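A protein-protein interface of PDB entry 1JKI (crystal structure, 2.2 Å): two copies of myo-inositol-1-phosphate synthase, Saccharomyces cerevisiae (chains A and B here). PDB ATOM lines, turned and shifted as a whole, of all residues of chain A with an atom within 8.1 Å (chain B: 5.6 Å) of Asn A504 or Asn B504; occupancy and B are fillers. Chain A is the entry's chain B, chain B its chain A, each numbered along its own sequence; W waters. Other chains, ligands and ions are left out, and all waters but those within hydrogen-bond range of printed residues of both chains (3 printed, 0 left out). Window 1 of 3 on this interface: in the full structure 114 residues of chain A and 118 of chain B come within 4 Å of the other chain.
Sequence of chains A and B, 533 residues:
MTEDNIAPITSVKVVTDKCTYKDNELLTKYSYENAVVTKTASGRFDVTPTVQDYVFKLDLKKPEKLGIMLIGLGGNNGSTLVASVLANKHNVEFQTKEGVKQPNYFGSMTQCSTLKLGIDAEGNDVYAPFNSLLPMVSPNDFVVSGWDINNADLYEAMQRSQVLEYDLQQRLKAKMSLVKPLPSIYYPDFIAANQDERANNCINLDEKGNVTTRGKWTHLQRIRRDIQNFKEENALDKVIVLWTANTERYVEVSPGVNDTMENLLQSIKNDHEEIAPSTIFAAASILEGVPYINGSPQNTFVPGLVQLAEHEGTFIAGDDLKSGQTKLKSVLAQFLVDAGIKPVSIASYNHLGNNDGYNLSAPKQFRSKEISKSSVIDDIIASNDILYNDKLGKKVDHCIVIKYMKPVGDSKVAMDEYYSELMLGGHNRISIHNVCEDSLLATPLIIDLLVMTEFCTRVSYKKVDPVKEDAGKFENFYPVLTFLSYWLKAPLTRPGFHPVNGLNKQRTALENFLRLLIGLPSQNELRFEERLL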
ATOM      1  N   LYS A 322     -15.061  38.742  28.618  1.00  0.00           N
ATOM      2  CA  LYS A 322     -15.824  37.602  29.132  1.00  0.00           C
ATOM      3  C   LYS A 322     -15.001  37.033  30.198  1.00  0.00           C
ATOM      4  O   LYS A 322     -14.051  36.244  30.043  1.00  0.00           O
ATOM      5  CB  LYS A 322     -16.159  36.554  28.085  1.00  0.00           C
ATOM      6  CG  LYS A 322     -17.679  36.659  27.676  1.00  0.00           C
ATOM      7  CD  LYS A 322     -18.292  35.253  27.531  1.00  0.00           C
ATOM      8  CE  LYS A 322     -19.743  35.300  27.197  1.00  0.00           C
ATOM      9  NZ  LYS A 322     -20.175  36.107  26.070  1.00  0.00           N
ATOM     10  N   LYS A 327     -18.634  32.846  32.003  1.00  0.00           N
ATOM     11  CA  LYS A 327     -18.828  31.921  30.937  1.00  0.00           C
ATOM     12  C   LYS A 327     -19.566  30.668  31.484  1.00  0.00           C
ATOM     13  O   LYS A 327     -20.662  30.331  31.048  1.00  0.00           O
ATOM     14  CB  LYS A 327     -17.446  31.486  30.361  1.00  0.00           C
ATOM     15  CG  LYS A 327     -16.970  32.219  29.009  1.00  0.00           C
ATOM     16  CD  LYS A 327     -15.362  32.007  28.680  1.00  0.00           C
ATOM     17  CE  LYS A 327     -14.850  30.927  27.627  1.00  0.00           C
ATOM     18  NZ  LYS A 327     -13.631  31.454  26.752  1.00  0.00           N
ATOM     19  N   SER A 330     -23.279  31.132  32.492  1.00  0.00           N
ATOM     20  CA  SER A 330     -24.306  31.133  31.399  1.00  0.00           C
ATOM     21  C   SER A 330     -24.422  29.672  30.902  1.00  0.00           C
ATOM     22  O   SER A 330     -25.497  29.146  30.691  1.00  0.00           O
ATOM     23  CB  SER A 330     -23.861  32.040  30.187  1.00  0.00           C
ATOM     24  OG  SER A 330     -24.433  33.365  30.098  1.00  0.00           O
ATOM     25  N   VAL A 331     -23.326  28.994  30.786  1.00  0.00           N
ATOM     26  CA  VAL A 331     -23.436  27.647  30.315  1.00  0.00           C
ATOM     27  C   VAL A 331     -24.252  26.799  31.293  1.00  0.00           C
ATOM     28  O   VAL A 331     -25.253  26.216  30.904  1.00  0.00           O
ATOM     29  CB  VAL A 331     -22.082  27.170  30.084  1.00  0.00           C
ATOM     30  CG1 VAL A 331     -21.971  25.725  30.089  1.00  0.00           C
ATOM     31  CG2 VAL A 331     -21.672  27.799  28.723  1.00  0.00           C
ATOM     32  N   LEU A 332     -23.766  26.660  32.540  1.00  0.00           N
ATOM     33  CA  LEU A 332     -24.521  26.005  33.644  1.00  0.00           C
ATOM     34  C   LEU A 332     -26.027  26.341  33.600  1.00  0.00           C
ATOM     35  O   LEU A 332     -26.850  25.504  33.543  1.00  0.00           O
ATOM     36  CB  LEU A 332     -23.999  26.515  34.974  1.00  0.00           C
ATOM     37  CG  LEU A 332     -23.129  25.385  35.395  1.00  0.00           C
ATOM     38  CD1 LEU A 332     -23.953  24.251  36.206  1.00  0.00           C
ATOM     39  CD2 LEU A 332     -22.604  24.731  34.026  1.00  0.00           C
ATOM     40  N   GLN A 334     -27.792  27.587  31.225  1.00  0.00           N
ATOM     41  CA  GLN A 334     -28.491  27.121  30.102  1.00  0.00           C
ATOM     42  C   GLN A 334     -28.712  25.650  30.206  1.00  0.00           C
ATOM     43  O   GLN A 334     -29.748  25.189  29.767  1.00  0.00           O
ATOM     44  CB  GLN A 334     -27.734  27.394  28.806  1.00  0.00           C
ATOM     45  CG  GLN A 334     -28.609  27.213  27.499  1.00  0.00           C
ATOM     46  CD  GLN A 334     -29.765  28.190  27.458  1.00  0.00           C
ATOM     47  OE1 GLN A 334     -30.896  27.797  27.164  1.00  0.00           O
ATOM     48  NE2 GLN A 334     -29.501  29.473  27.763  1.00  0.00           N
ATOM     49  N   PHE A 335     -27.754  24.884  30.695  1.00  0.00           N
ATOM     50  CA  PHE A 335     -28.014  23.475  30.779  1.00  0.00           C
ATOM     51  C   PHE A 335     -29.275  23.049  31.611  1.00  0.00           C
ATOM     52  O   PHE A 335     -29.866  22.050  31.349  1.00  0.00           O
ATOM     53  CB  PHE A 335     -26.791  22.796  31.301  1.00  0.00           C
ATOM     54  CG  PHE A 335     -27.023  21.423  31.911  1.00  0.00           C
ATOM     55  CD1 PHE A 335     -27.382  21.280  33.260  1.00  0.00           C
ATOM     56  CD2 PHE A 335     -26.794  20.276  31.196  1.00  0.00           C
ATOM     57  CE1 PHE A 335     -27.508  20.008  33.873  1.00  0.00           C
ATOM     58  CE2 PHE A 335     -26.921  18.939  31.829  1.00  0.00           C
ATOM     59  CZ  PHE A 335     -27.276  18.819  33.144  1.00  0.00           C
ATOM     60  N   LEU A 336     -29.623  23.882  32.587  1.00  0.00           N
ATOM     61  CA  LEU A 336     -30.632  23.662  33.573  1.00  0.00           C
ATOM     62  C   LEU A 336     -31.942  24.019  32.841  1.00  0.00           C
ATOM     63  O   LEU A 336     -32.852  23.240  32.826  1.00  0.00           O
ATOM     64  CB  LEU A 336     -30.294  24.561  34.818  1.00  0.00           C
ATOM     65  CG  LEU A 336     -29.116  24.206  35.874  1.00  0.00           C
ATOM     66  CD1 LEU A 336     -29.055  25.175  37.123  1.00  0.00           C
ATOM     67  CD2 LEU A 336     -29.219  22.848  36.430  1.00  0.00           C
ATOM     68  N   ASP A 338     -32.591  24.038  29.671  1.00  0.00           N
ATOM     69  CA  ASP A 338     -32.740  23.078  28.608  1.00  0.00           C
ATOM     70  C   ASP A 338     -33.146  21.659  29.098  1.00  0.00           C
ATOM     71  O   ASP A 338     -33.540  20.802  28.246  1.00  0.00           O
ATOM     72  CB  ASP A 338     -31.408  22.825  27.891  1.00  0.00           C
ATOM     73  CG  ASP A 338     -30.944  23.954  26.984  1.00  0.00           C
ATOM     74  OD1 ASP A 338     -29.741  23.739  26.626  1.00  0.00           O
ATOM     75  OD2 ASP A 338     -31.624  24.992  26.658  1.00  0.00           O
ATOM     76  N   TYR A 486     -18.606  35.767  21.947  1.00  0.00           N
ATOM     77  CA  TYR A 486     -18.178  34.626  22.711  1.00  0.00           C
ATOM     78  C   TYR A 486     -17.217  34.986  23.838  1.00  0.00           C
ATOM     79  O   TYR A 486     -16.997  34.195  24.787  1.00  0.00           O
ATOM     80  CB  TYR A 486     -17.369  33.664  21.858  1.00  0.00           C
ATOM     81  CG  TYR A 486     -16.815  32.531  22.687  1.00  0.00           C
ATOM     82  CD1 TYR A 486     -17.585  31.340  22.919  1.00  0.00           C
ATOM     83  CD2 TYR A 486     -15.484  32.576  23.159  1.00  0.00           C
ATOM     84  CE1 TYR A 486     -16.993  30.202  23.568  1.00  0.00           C
ATOM     85  CE2 TYR A 486     -14.899  31.490  23.803  1.00  0.00           C
ATOM     86  CZ  TYR A 486     -15.638  30.297  23.986  1.00  0.00           C
ATOM     87  OH  TYR A 486     -14.928  29.202  24.382  1.00  0.00           O
ATOM     88  N   ASN A 501     -26.587  36.075  24.485  1.00  0.00           N
ATOM     89  CA  ASN A 501     -25.343  35.505  24.957  1.00  0.00           C
ATOM     90  C   ASN A 501     -25.633  33.983  24.878  1.00  0.00           C
ATOM     91  O   ASN A 501     -26.567  33.577  24.177  1.00  0.00           O
ATOM     92  CB  ASN A 501     -25.074  36.075  26.378  1.00  0.00           C
ATOM     93  CG  ASN A 501     -24.811  37.649  26.361  1.00  0.00           C
ATOM     94  OD1 ASN A 501     -23.764  38.151  26.871  1.00  0.00           O
ATOM     95  ND2 ASN A 501     -25.758  38.404  25.788  1.00  0.00           N
ATOM     96  N   GLY A 502     -24.920  33.110  25.569  1.00  0.00           N
ATOM     97  CA  GLY A 502     -25.238  31.692  25.359  1.00  0.00           C
ATOM     98  C   GLY A 502     -23.940  31.424  24.645  1.00  0.00           C
ATOM     99  O   GLY A 502     -23.810  31.463  23.402  1.00  0.00           O
ATOM    100  N   LEU A 503     -22.933  31.263  25.491  1.00  0.00           N
ATOM    101  CA  LEU A 503     -21.571  31.040  25.024  1.00  0.00           C
ATOM    102  C   LEU A 503     -21.553  30.008  23.933  1.00  0.00           C
ATOM    103  O   LEU A 503     -21.085  30.328  22.851  1.00  0.00           O
ATOM    104  CB  LEU A 503     -20.620  30.562  26.163  1.00  0.00           C
ATOM    105  CG  LEU A 503     -19.120  30.638  25.747  1.00  0.00           C
ATOM    106  CD1 LEU A 503     -18.578  32.025  26.102  1.00  0.00           C
ATOM    107  CD2 LEU A 503     -18.282  29.458  26.349  1.00  0.00           C
ATOM    108  N   ASN A 504     -22.073  28.800  24.244  1.00  0.00           N
ATOM    109  CA  ASN A 504     -22.055  27.616  23.341  1.00  0.00           C
ATOM    110  C   ASN A 504     -22.468  27.949  21.900  1.00  0.00           C
ATOM    111  O   ASN A 504     -21.685  27.686  20.959  1.00  0.00           O
ATOM    112  CB  ASN A 504     -22.859  26.416  23.922  1.00  0.00           C
ATOM    113  CG  ASN A 504     -21.961  25.470  24.769  1.00  0.00           C
ATOM    114  OD1 ASN A 504     -22.133  24.186  24.794  1.00  0.00           O
ATOM    115  ND2 ASN A 504     -20.981  26.083  25.470  1.00  0.00           N
ATOM    116  N   LYS A 505     -23.674  28.536  21.800  1.00  0.00           N
ATOM    117  CA  LYS A 505     -24.298  29.039  20.624  1.00  0.00           C
ATOM    118  C   LYS A 505     -23.366  30.144  20.007  1.00  0.00           C
ATOM    119  O   LYS A 505     -23.276  30.271  18.740  1.00  0.00           O
ATOM    120  CB  LYS A 505     -25.653  29.646  21.016  1.00  0.00           C
ATOM    121  CG  LYS A 505     -26.695  28.587  21.378  1.00  0.00           C
ATOM    122  CD  LYS A 505     -28.004  29.255  21.657  1.00  0.00           C
ATOM    123  CE  LYS A 505     -27.768  30.630  22.307  1.00  0.00           C
ATOM    124  NZ  LYS A 505     -29.065  31.494  22.522  1.00  0.00           N
ATOM    125  N   GLN A 506     -22.712  30.959  20.864  1.00  0.00           N
ATOM    126  CA  GLN A 506     -21.805  31.967  20.381  1.00  0.00           C
ATOM    127  C   GLN A 506     -20.693  31.205  19.747  1.00  0.00           C
ATOM    128  O   GLN A 506     -20.111  31.674  18.741  1.00  0.00           O
ATOM    129  CB  GLN A 506     -21.225  32.824  21.480  1.00  0.00           C
ATOM    130  CG  GLN A 506     -22.042  34.049  21.818  1.00  0.00           C
ATOM    131  CD  GLN A 506     -21.779  34.629  23.260  1.00  0.00           C
ATOM    132  OE1 GLN A 506     -22.322  35.677  23.575  1.00  0.00           O
ATOM    133  NE2 GLN A 506     -20.952  33.938  24.107  1.00  0.00           N
ATOM    134  N   ARG A 507     -20.374  30.012  20.268  1.00  0.00           N
ATOM    135  CA  ARG A 507     -19.293  29.294  19.597  1.00  0.00           C
ATOM    136  C   ARG A 507     -19.657  28.514  18.274  1.00  0.00           C
ATOM    137  O   ARG A 507     -18.784  28.271  17.380  1.00  0.00           O
ATOM    138  CB  ARG A 507     -18.606  28.352  20.540  1.00  0.00           C
ATOM    139  CG  ARG A 507     -17.260  28.201  20.000  1.00  0.00           C
ATOM    140  CD  ARG A 507     -16.433  27.339  20.764  1.00  0.00           C
ATOM    141  NE  ARG A 507     -16.493  26.046  20.167  1.00  0.00           N
ATOM    142  CZ  ARG A 507     -15.418  25.309  19.955  1.00  0.00           C
ATOM    143  NH1 ARG A 507     -14.263  25.879  20.320  1.00  0.00           N
ATOM    144  NH2 ARG A 507     -15.509  24.015  19.435  1.00  0.00           N
ATOM    145  N   THR A 508     -20.914  28.074  18.212  1.00  0.00           N
ATOM    146  CA  THR A 508     -21.470  27.394  17.063  1.00  0.00           C
ATOM    147  C   THR A 508     -21.369  28.392  15.885  1.00  0.00           C
ATOM    148  O   THR A 508     -20.884  28.049  14.838  1.00  0.00           O
ATOM    149  CB  THR A 508     -22.936  26.923  17.388  1.00  0.00           C
ATOM    150  OG1 THR A 508     -22.830  25.803  18.221  1.00  0.00           O
ATOM    151  CG2 THR A 508     -23.697  26.449  16.162  1.00  0.00           C
ATOM    152  N   ALA A 509     -21.746  29.631  16.144  1.00  0.00           N
ATOM    153  CA  ALA A 509     -21.665  30.678  15.168  1.00  0.00           C
ATOM    154  C   ALA A 509     -20.315  30.721  14.479  1.00  0.00           C
ATOM    155  O   ALA A 509     -20.270  30.676  13.248  1.00  0.00           O
ATOM    156  CB  ALA A 509     -21.938  32.007  15.766  1.00  0.00           C
ATOM    157  N   LEU A 510     -19.208  30.781  15.227  1.00  0.00           N
ATOM    158  CA  LEU A 510     -17.865  30.905  14.589  1.00  0.00           C
ATOM    159  C   LEU A 510     -17.497  29.762  13.741  1.00  0.00           C
ATOM    160  O   LEU A 510     -16.815  29.833  12.722  1.00  0.00           O
ATOM    161  CB  LEU A 510     -16.746  30.963  15.649  1.00  0.00           C
ATOM    162  CG  LEU A 510     -16.181  32.221  16.249  1.00  0.00           C
ATOM    163  CD1 LEU A 510     -14.812  32.532  15.442  1.00  0.00           C
ATOM    164  CD2 LEU A 510     -17.187  33.373  16.261  1.00  0.00           C
ATOM    165  N   GLU A 511     -17.747  28.679  14.383  1.00  0.00           N
ATOM    166  CA  GLU A 511     -17.415  27.427  13.848  1.00  0.00           C
ATOM    167  C   GLU A 511     -18.113  27.207  12.418  1.00  0.00           C
ATOM    168  O   GLU A 511     -17.452  26.779  11.454  1.00  0.00           O
ATOM    169  CB  GLU A 511     -17.875  26.433  14.857  1.00  0.00           C
ATOM    170  CG  GLU A 511     -17.237  25.175  14.732  1.00  0.00           C
ATOM    171  CD  GLU A 511     -18.269  24.071  14.972  1.00  0.00           C
ATOM    172  OE1 GLU A 511     -18.002  22.833  14.896  1.00  0.00           O
ATOM    173  OE2 GLU A 511     -19.398  24.526  15.246  1.00  0.00           O
ATOM    174  N   ASN A 524     -24.986  19.128  12.261  1.00  0.00           N
ATOM    175  CA  ASN A 524     -26.375  18.933  12.672  1.00  0.00           C
ATOM    176  C   ASN A 524     -26.528  17.859  13.763  1.00  0.00           C
ATOM    177  O   ASN A 524     -27.579  17.877  14.396  1.00  0.00           O
ATOM    178  CB  ASN A 524     -27.323  18.629  11.455  1.00  0.00           C
ATOM    179  CG  ASN A 524     -26.800  17.488  10.564  1.00  0.00           C
ATOM    180  OD1 ASN A 524     -26.427  16.399  11.037  1.00  0.00           O
ATOM    181  ND2 ASN A 524     -26.730  17.777   9.208  1.00  0.00           N
ATOM    182  N   GLU A 525     -25.526  16.980  13.925  1.00  0.00           N
ATOM    183  CA  GLU A 525     -25.415  15.936  14.884  1.00  0.00           C
ATOM    184  C   GLU A 525     -26.290  14.792  14.755  1.00  0.00           C
ATOM    185  O   GLU A 525     -26.329  13.934  15.730  1.00  0.00           O
ATOM    186  CB  GLU A 525     -25.646  16.367  16.354  1.00  0.00           C
ATOM    187  CG  GLU A 525     -24.858  17.551  16.802  1.00  0.00           C
ATOM    188  CD  GLU A 525     -23.405  17.204  16.755  1.00  0.00           C
ATOM    189  OE1 GLU A 525     -22.656  18.183  16.513  1.00  0.00           O
ATOM    190  OE2 GLU A 525     -23.026  15.956  16.950  1.00  0.00           O
ATOM    191  N   VAL B 331     -21.018  18.527  30.319  1.00  0.00           N
ATOM    192  CA  VAL B 331     -21.188  19.864  29.863  1.00  0.00           C
ATOM    193  C   VAL B 331     -19.862  20.661  30.216  1.00  0.00           C
ATOM    194  O   VAL B 331     -19.152  21.339  29.385  1.00  0.00           O
ATOM    195  CB  VAL B 331     -22.401  20.343  30.578  1.00  0.00           C
ATOM    196  CG1 VAL B 331     -22.661  21.797  30.431  1.00  0.00           C
ATOM    197  CG2 VAL B 331     -23.519  19.520  30.072  1.00  0.00           C
ATOM    198  N   GLN B 334     -16.395  19.678  28.554  1.00  0.00           N
ATOM    199  CA  GLN B 334     -16.396  20.043  27.168  1.00  0.00           C
ATOM    200  C   GLN B 334     -16.187  21.556  27.028  1.00  0.00           C
ATOM    201  O   GLN B 334     -15.434  21.978  26.202  1.00  0.00           O
ATOM    202  CB  GLN B 334     -17.799  19.651  26.481  1.00  0.00           C
ATOM    203  CG  GLN B 334     -17.710  19.542  24.898  1.00  0.00           C
ATOM    204  CD  GLN B 334     -16.756  18.434  24.505  1.00  0.00           C
ATOM    205  OE1 GLN B 334     -15.682  18.677  23.884  1.00  0.00           O
ATOM    206  NE2 GLN B 334     -17.117  17.190  24.892  1.00  0.00           N
ATOM    207  N   PHE B 335     -16.946  22.332  27.768  1.00  0.00           N
ATOM    208  CA  PHE B 335     -16.776  23.717  27.795  1.00  0.00           C
ATOM    209  C   PHE B 335     -15.177  24.054  27.968  1.00  0.00           C
ATOM    210  O   PHE B 335     -14.616  24.767  27.204  1.00  0.00           O
ATOM    211  CB  PHE B 335     -17.481  24.222  28.976  1.00  0.00           C
ATOM    212  CG  PHE B 335     -17.033  25.617  29.407  1.00  0.00           C
ATOM    213  CD1 PHE B 335     -17.432  26.729  28.724  1.00  0.00           C
ATOM    214  CD2 PHE B 335     -16.269  25.797  30.579  1.00  0.00           C
ATOM    215  CE1 PHE B 335     -17.094  28.034  29.191  1.00  0.00           C
ATOM    216  CE2 PHE B 335     -15.936  27.071  31.020  1.00  0.00           C
ATOM    217  CZ  PHE B 335     -16.350  28.203  30.332  1.00  0.00           C
ATOM    218  N   ASP B 338     -13.262  23.009  24.929  1.00  0.00           N
ATOM    219  CA  ASP B 338     -13.484  23.749  23.702  1.00  0.00           C
ATOM    220  C   ASP B 338     -12.879  25.104  23.878  1.00  0.00           C
ATOM    221  O   ASP B 338     -12.928  25.999  22.911  1.00  0.00           O
ATOM    222  CB  ASP B 338     -14.995  24.135  23.411  1.00  0.00           C
ATOM    223  CG  ASP B 338     -15.980  22.946  23.148  1.00  0.00           C
ATOM    224  OD1 ASP B 338     -17.204  23.302  22.969  1.00  0.00           O
ATOM    225  OD2 ASP B 338     -15.595  21.748  23.097  1.00  0.00           O
ATOM    226  N   GLY B 502     -21.203  13.916  24.386  1.00  0.00           N
ATOM    227  CA  GLY B 502     -21.367  15.353  24.547  1.00  0.00           C
ATOM    228  C   GLY B 502     -22.767  15.789  24.863  1.00  0.00           C
ATOM    229  O   GLY B 502     -23.586  15.957  23.932  1.00  0.00           O
ATOM    230  N   LEU B 503     -23.083  16.050  26.123  1.00  0.00           N
ATOM    231  CA  LEU B 503     -24.482  16.420  26.389  1.00  0.00           C
ATOM    232  C   LEU B 503     -25.159  17.381  25.393  1.00  0.00           C
ATOM    233  O   LEU B 503     -26.245  17.088  24.889  1.00  0.00           O
ATOM    234  CB  LEU B 503     -24.708  17.031  27.776  1.00  0.00           C
ATOM    235  CG  LEU B 503     -26.247  16.917  28.111  1.00  0.00           C
ATOM    236  CD1 LEU B 503     -26.504  15.522  28.707  1.00  0.00           C
ATOM    237  CD2 LEU B 503     -26.723  17.918  29.082  1.00  0.00           C
ATOM    238  N   ASN B 504     -24.559  18.544  25.145  1.00  0.00           N
ATOM    239  CA  ASN B 504     -25.213  19.525  24.298  1.00  0.00           C
ATOM    240  C   ASN B 504     -25.367  19.097  22.843  1.00  0.00           C
ATOM    241  O   ASN B 504     -26.255  19.578  22.101  1.00  0.00           O
ATOM    242  CB  ASN B 504     -24.483  20.838  24.413  1.00  0.00           C
ATOM    243  CG  ASN B 504     -24.292  21.249  25.848  1.00  0.00           C
ATOM    244  OD1 ASN B 504     -25.260  21.728  26.506  1.00  0.00           O
ATOM    245  ND2 ASN B 504     -23.053  21.069  26.366  1.00  0.00           N
ATOM    246  N   LYS B 505     -24.517  18.153  22.455  1.00  0.00           N
ATOM    247  CA  LYS B 505     -24.558  17.654  21.119  1.00  0.00           C
ATOM    248  C   LYS B 505     -25.669  16.601  20.913  1.00  0.00           C
ATOM    249  O   LYS B 505     -26.205  16.502  19.784  1.00  0.00           O
ATOM    250  CB  LYS B 505     -23.160  17.167  20.723  1.00  0.00           C
ATOM    251  CG  LYS B 505     -22.422  18.338  19.938  1.00  0.00           C
ATOM    252  CD  LYS B 505     -20.870  18.415  20.041  1.00  0.00           C
ATOM    253  CE  LYS B 505     -20.131  17.077  19.707  1.00  0.00           C
ATOM    254  NZ  LYS B 505     -20.079  15.952  20.727  1.00  0.00           N
ATOM    255  N   GLN B 506     -26.041  15.874  21.989  1.00  0.00           N
ATOM    256  CA  GLN B 506     -27.078  14.876  21.966  1.00  0.00           C
ATOM    257  C   GLN B 506     -28.404  15.601  21.923  1.00  0.00           C
ATOM    258  O   GLN B 506     -29.343  15.146  21.290  1.00  0.00           O
ATOM    259  CB  GLN B 506     -27.026  14.055  23.202  1.00  0.00           C
ATOM    260  CG  GLN B 506     -25.961  13.024  23.152  1.00  0.00           C
ATOM    261  CD  GLN B 506     -25.508  12.578  24.554  1.00  0.00           C
ATOM    262  OE1 GLN B 506     -25.844  13.235  25.610  1.00  0.00           O
ATOM    263  NE2 GLN B 506     -24.802  11.475  24.581  1.00  0.00           N
ATOM    264  N   ARG B 507     -28.495  16.754  22.555  1.00  0.00           N
ATOM    265  CA  ARG B 507     -29.807  17.412  22.547  1.00  0.00           C
ATOM    266  C   ARG B 507     -30.031  18.102  21.177  1.00  0.00           C
ATOM    267  O   ARG B 507     -31.152  18.248  20.680  1.00  0.00           O
ATOM    268  CB  ARG B 507     -29.973  18.500  23.691  1.00  0.00           C
ATOM    269  CG  ARG B 507     -31.462  19.093  23.790  1.00  0.00           C
ATOM    270  CD  ARG B 507     -31.723  20.166  24.803  1.00  0.00           C
ATOM    271  NE  ARG B 507     -33.145  20.574  24.947  1.00  0.00           N
ATOM    272  CZ  ARG B 507     -33.574  21.728  24.474  1.00  0.00           C
ATOM    273  NH1 ARG B 507     -32.706  22.561  23.802  1.00  0.00           N
ATOM    274  NH2 ARG B 507     -34.828  22.130  24.679  1.00  0.00           N
ATOM    275  N   THR B 508     -28.958  18.632  20.646  1.00  0.00           N
ATOM    276  CA  THR B 508     -28.981  19.323  19.357  1.00  0.00           C
ATOM    277  C   THR B 508     -29.475  18.382  18.221  1.00  0.00           C
ATOM    278  O   THR B 508     -30.210  18.775  17.366  1.00  0.00           O
ATOM    279  CB  THR B 508     -27.585  19.853  19.062  1.00  0.00           C
ATOM    280  OG1 THR B 508     -27.456  20.982  19.905  1.00  0.00           O
ATOM    281  CG2 THR B 508     -27.502  20.341  17.593  1.00  0.00           C
ATOM    282  N   ALA B 509     -28.999  17.163  18.338  1.00  0.00           N
ATOM    283  CA  ALA B 509     -29.312  16.090  17.507  1.00  0.00           C
ATOM    284  C   ALA B 509     -30.854  15.828  17.537  1.00  0.00           C
ATOM    285  O   ALA B 509     -31.425  15.435  16.518  1.00  0.00           O
ATOM    286  CB  ALA B 509     -28.599  14.916  17.944  1.00  0.00           C
HETATM  287  O   HOH W   1     -20.621  22.229  27.068  1.00  0.00           O
HETATM  288  O   HOH W   2     -15.804  27.169  25.833  1.00  0.00           O
HETATM  289  O   HOH W   3     -18.655  22.975  20.389  1.00  0.00           O
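Phe A335 touches Val B331, but with the chains exchanged Val A331 does not touch Phe B335 (4.4 Å).
Phe A335 touches Leu B503, and with the chains exchanged Leu A503 touches Phe B335.
Asp A338 touches Arg B507, and with the chains exchanged Arg A507 touches Asp B338.
Asn B504 touches its own counterpart, Asn A504.
12 positions are printed for both chains.
The guanidinium group (NH1) of Arg B507 is in salt-bridge range of the side-chain carboxylate (OD2) of Asp A338, at 3.9 Å.
OD1 of Asp B338 lies within salt-bridge range of NH2 of Arg A507 (3.98 Å).
Hydrophobic or aromatic side chains of chain A that line the printed part of chain B: Phe A335 and Leu A503.
Of the 12 printed residues of chain B, 9 touch a printed residue of chain A.
Among the printed residues, 11 pairs touch across the chains.
Among the printed residues, Asp or Glu carboxylates within 4 Å of a Lys or Arg side-chain nitrogen of the other chain: Asp A338 with Arg B507 and Arg A507 with Asp B338.
Of chain B, only Asn B504 (3.6 Å) comes within 4 Å of Asn A504.
Printed residues of chain A within 4 Å of Asn B504: Asn A504.
Of the printed residues of chain B, Leu A503 touches Phe B335 (3.4 Å).
Of the printed residues of chain B, Arg A507 touches Asp B338 (2.9 Å).
The nearest residue of chain A that does not touch Asn B504 is Asp A338 (4.9 Å).
The backbone carbonyl oxygen (O) of Asn B504 sits at hydrogen-bond distance from the side-chain hydroxyl (OG1) of Thr B508, at 2.9 Å.
The side-chain amide oxygen (OE1) of Gln B334 lies close to the side-chain carboxylate (OD2) of Asp B338.
OE1 of Gln A334 lies close to OD2 of Asp A338.
Among the printed residues, merely in contact across the chains: Phe A335 with Leu B503 (2.9 Å), Glu A525 with Ala B509 (3.3 Å), Leu A503 with Phe B335 (3.4 Å), Glu A525 with Lys B505 (3.4 Å), Lys A327 with Phe B335 (3.5 Å), Phe A335 with Val B331 (3.5 Å), Asn A504 with Asn B504 (3.6 Å), Glu A525 with Thr B508 (3.9 Å) and Asn A524 with Ala B509 (3.98 Å).
Water W2 bridges OH of Tyr A486 (2.6 Å) and O of Phe B335 (3.0 Å).
Water W1 lies within hydrogen-bond range of ND2 of Asn B504 (2.8 Å), O of Val B331 (2.9 Å) and OD1 of Asn A504 (3.4 Å).
Water W3 lies within hydrogen-bond range of the side-chain carboxylate (OD1) of Asp B338 and the guanidinium group (NH2) of Arg A507.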
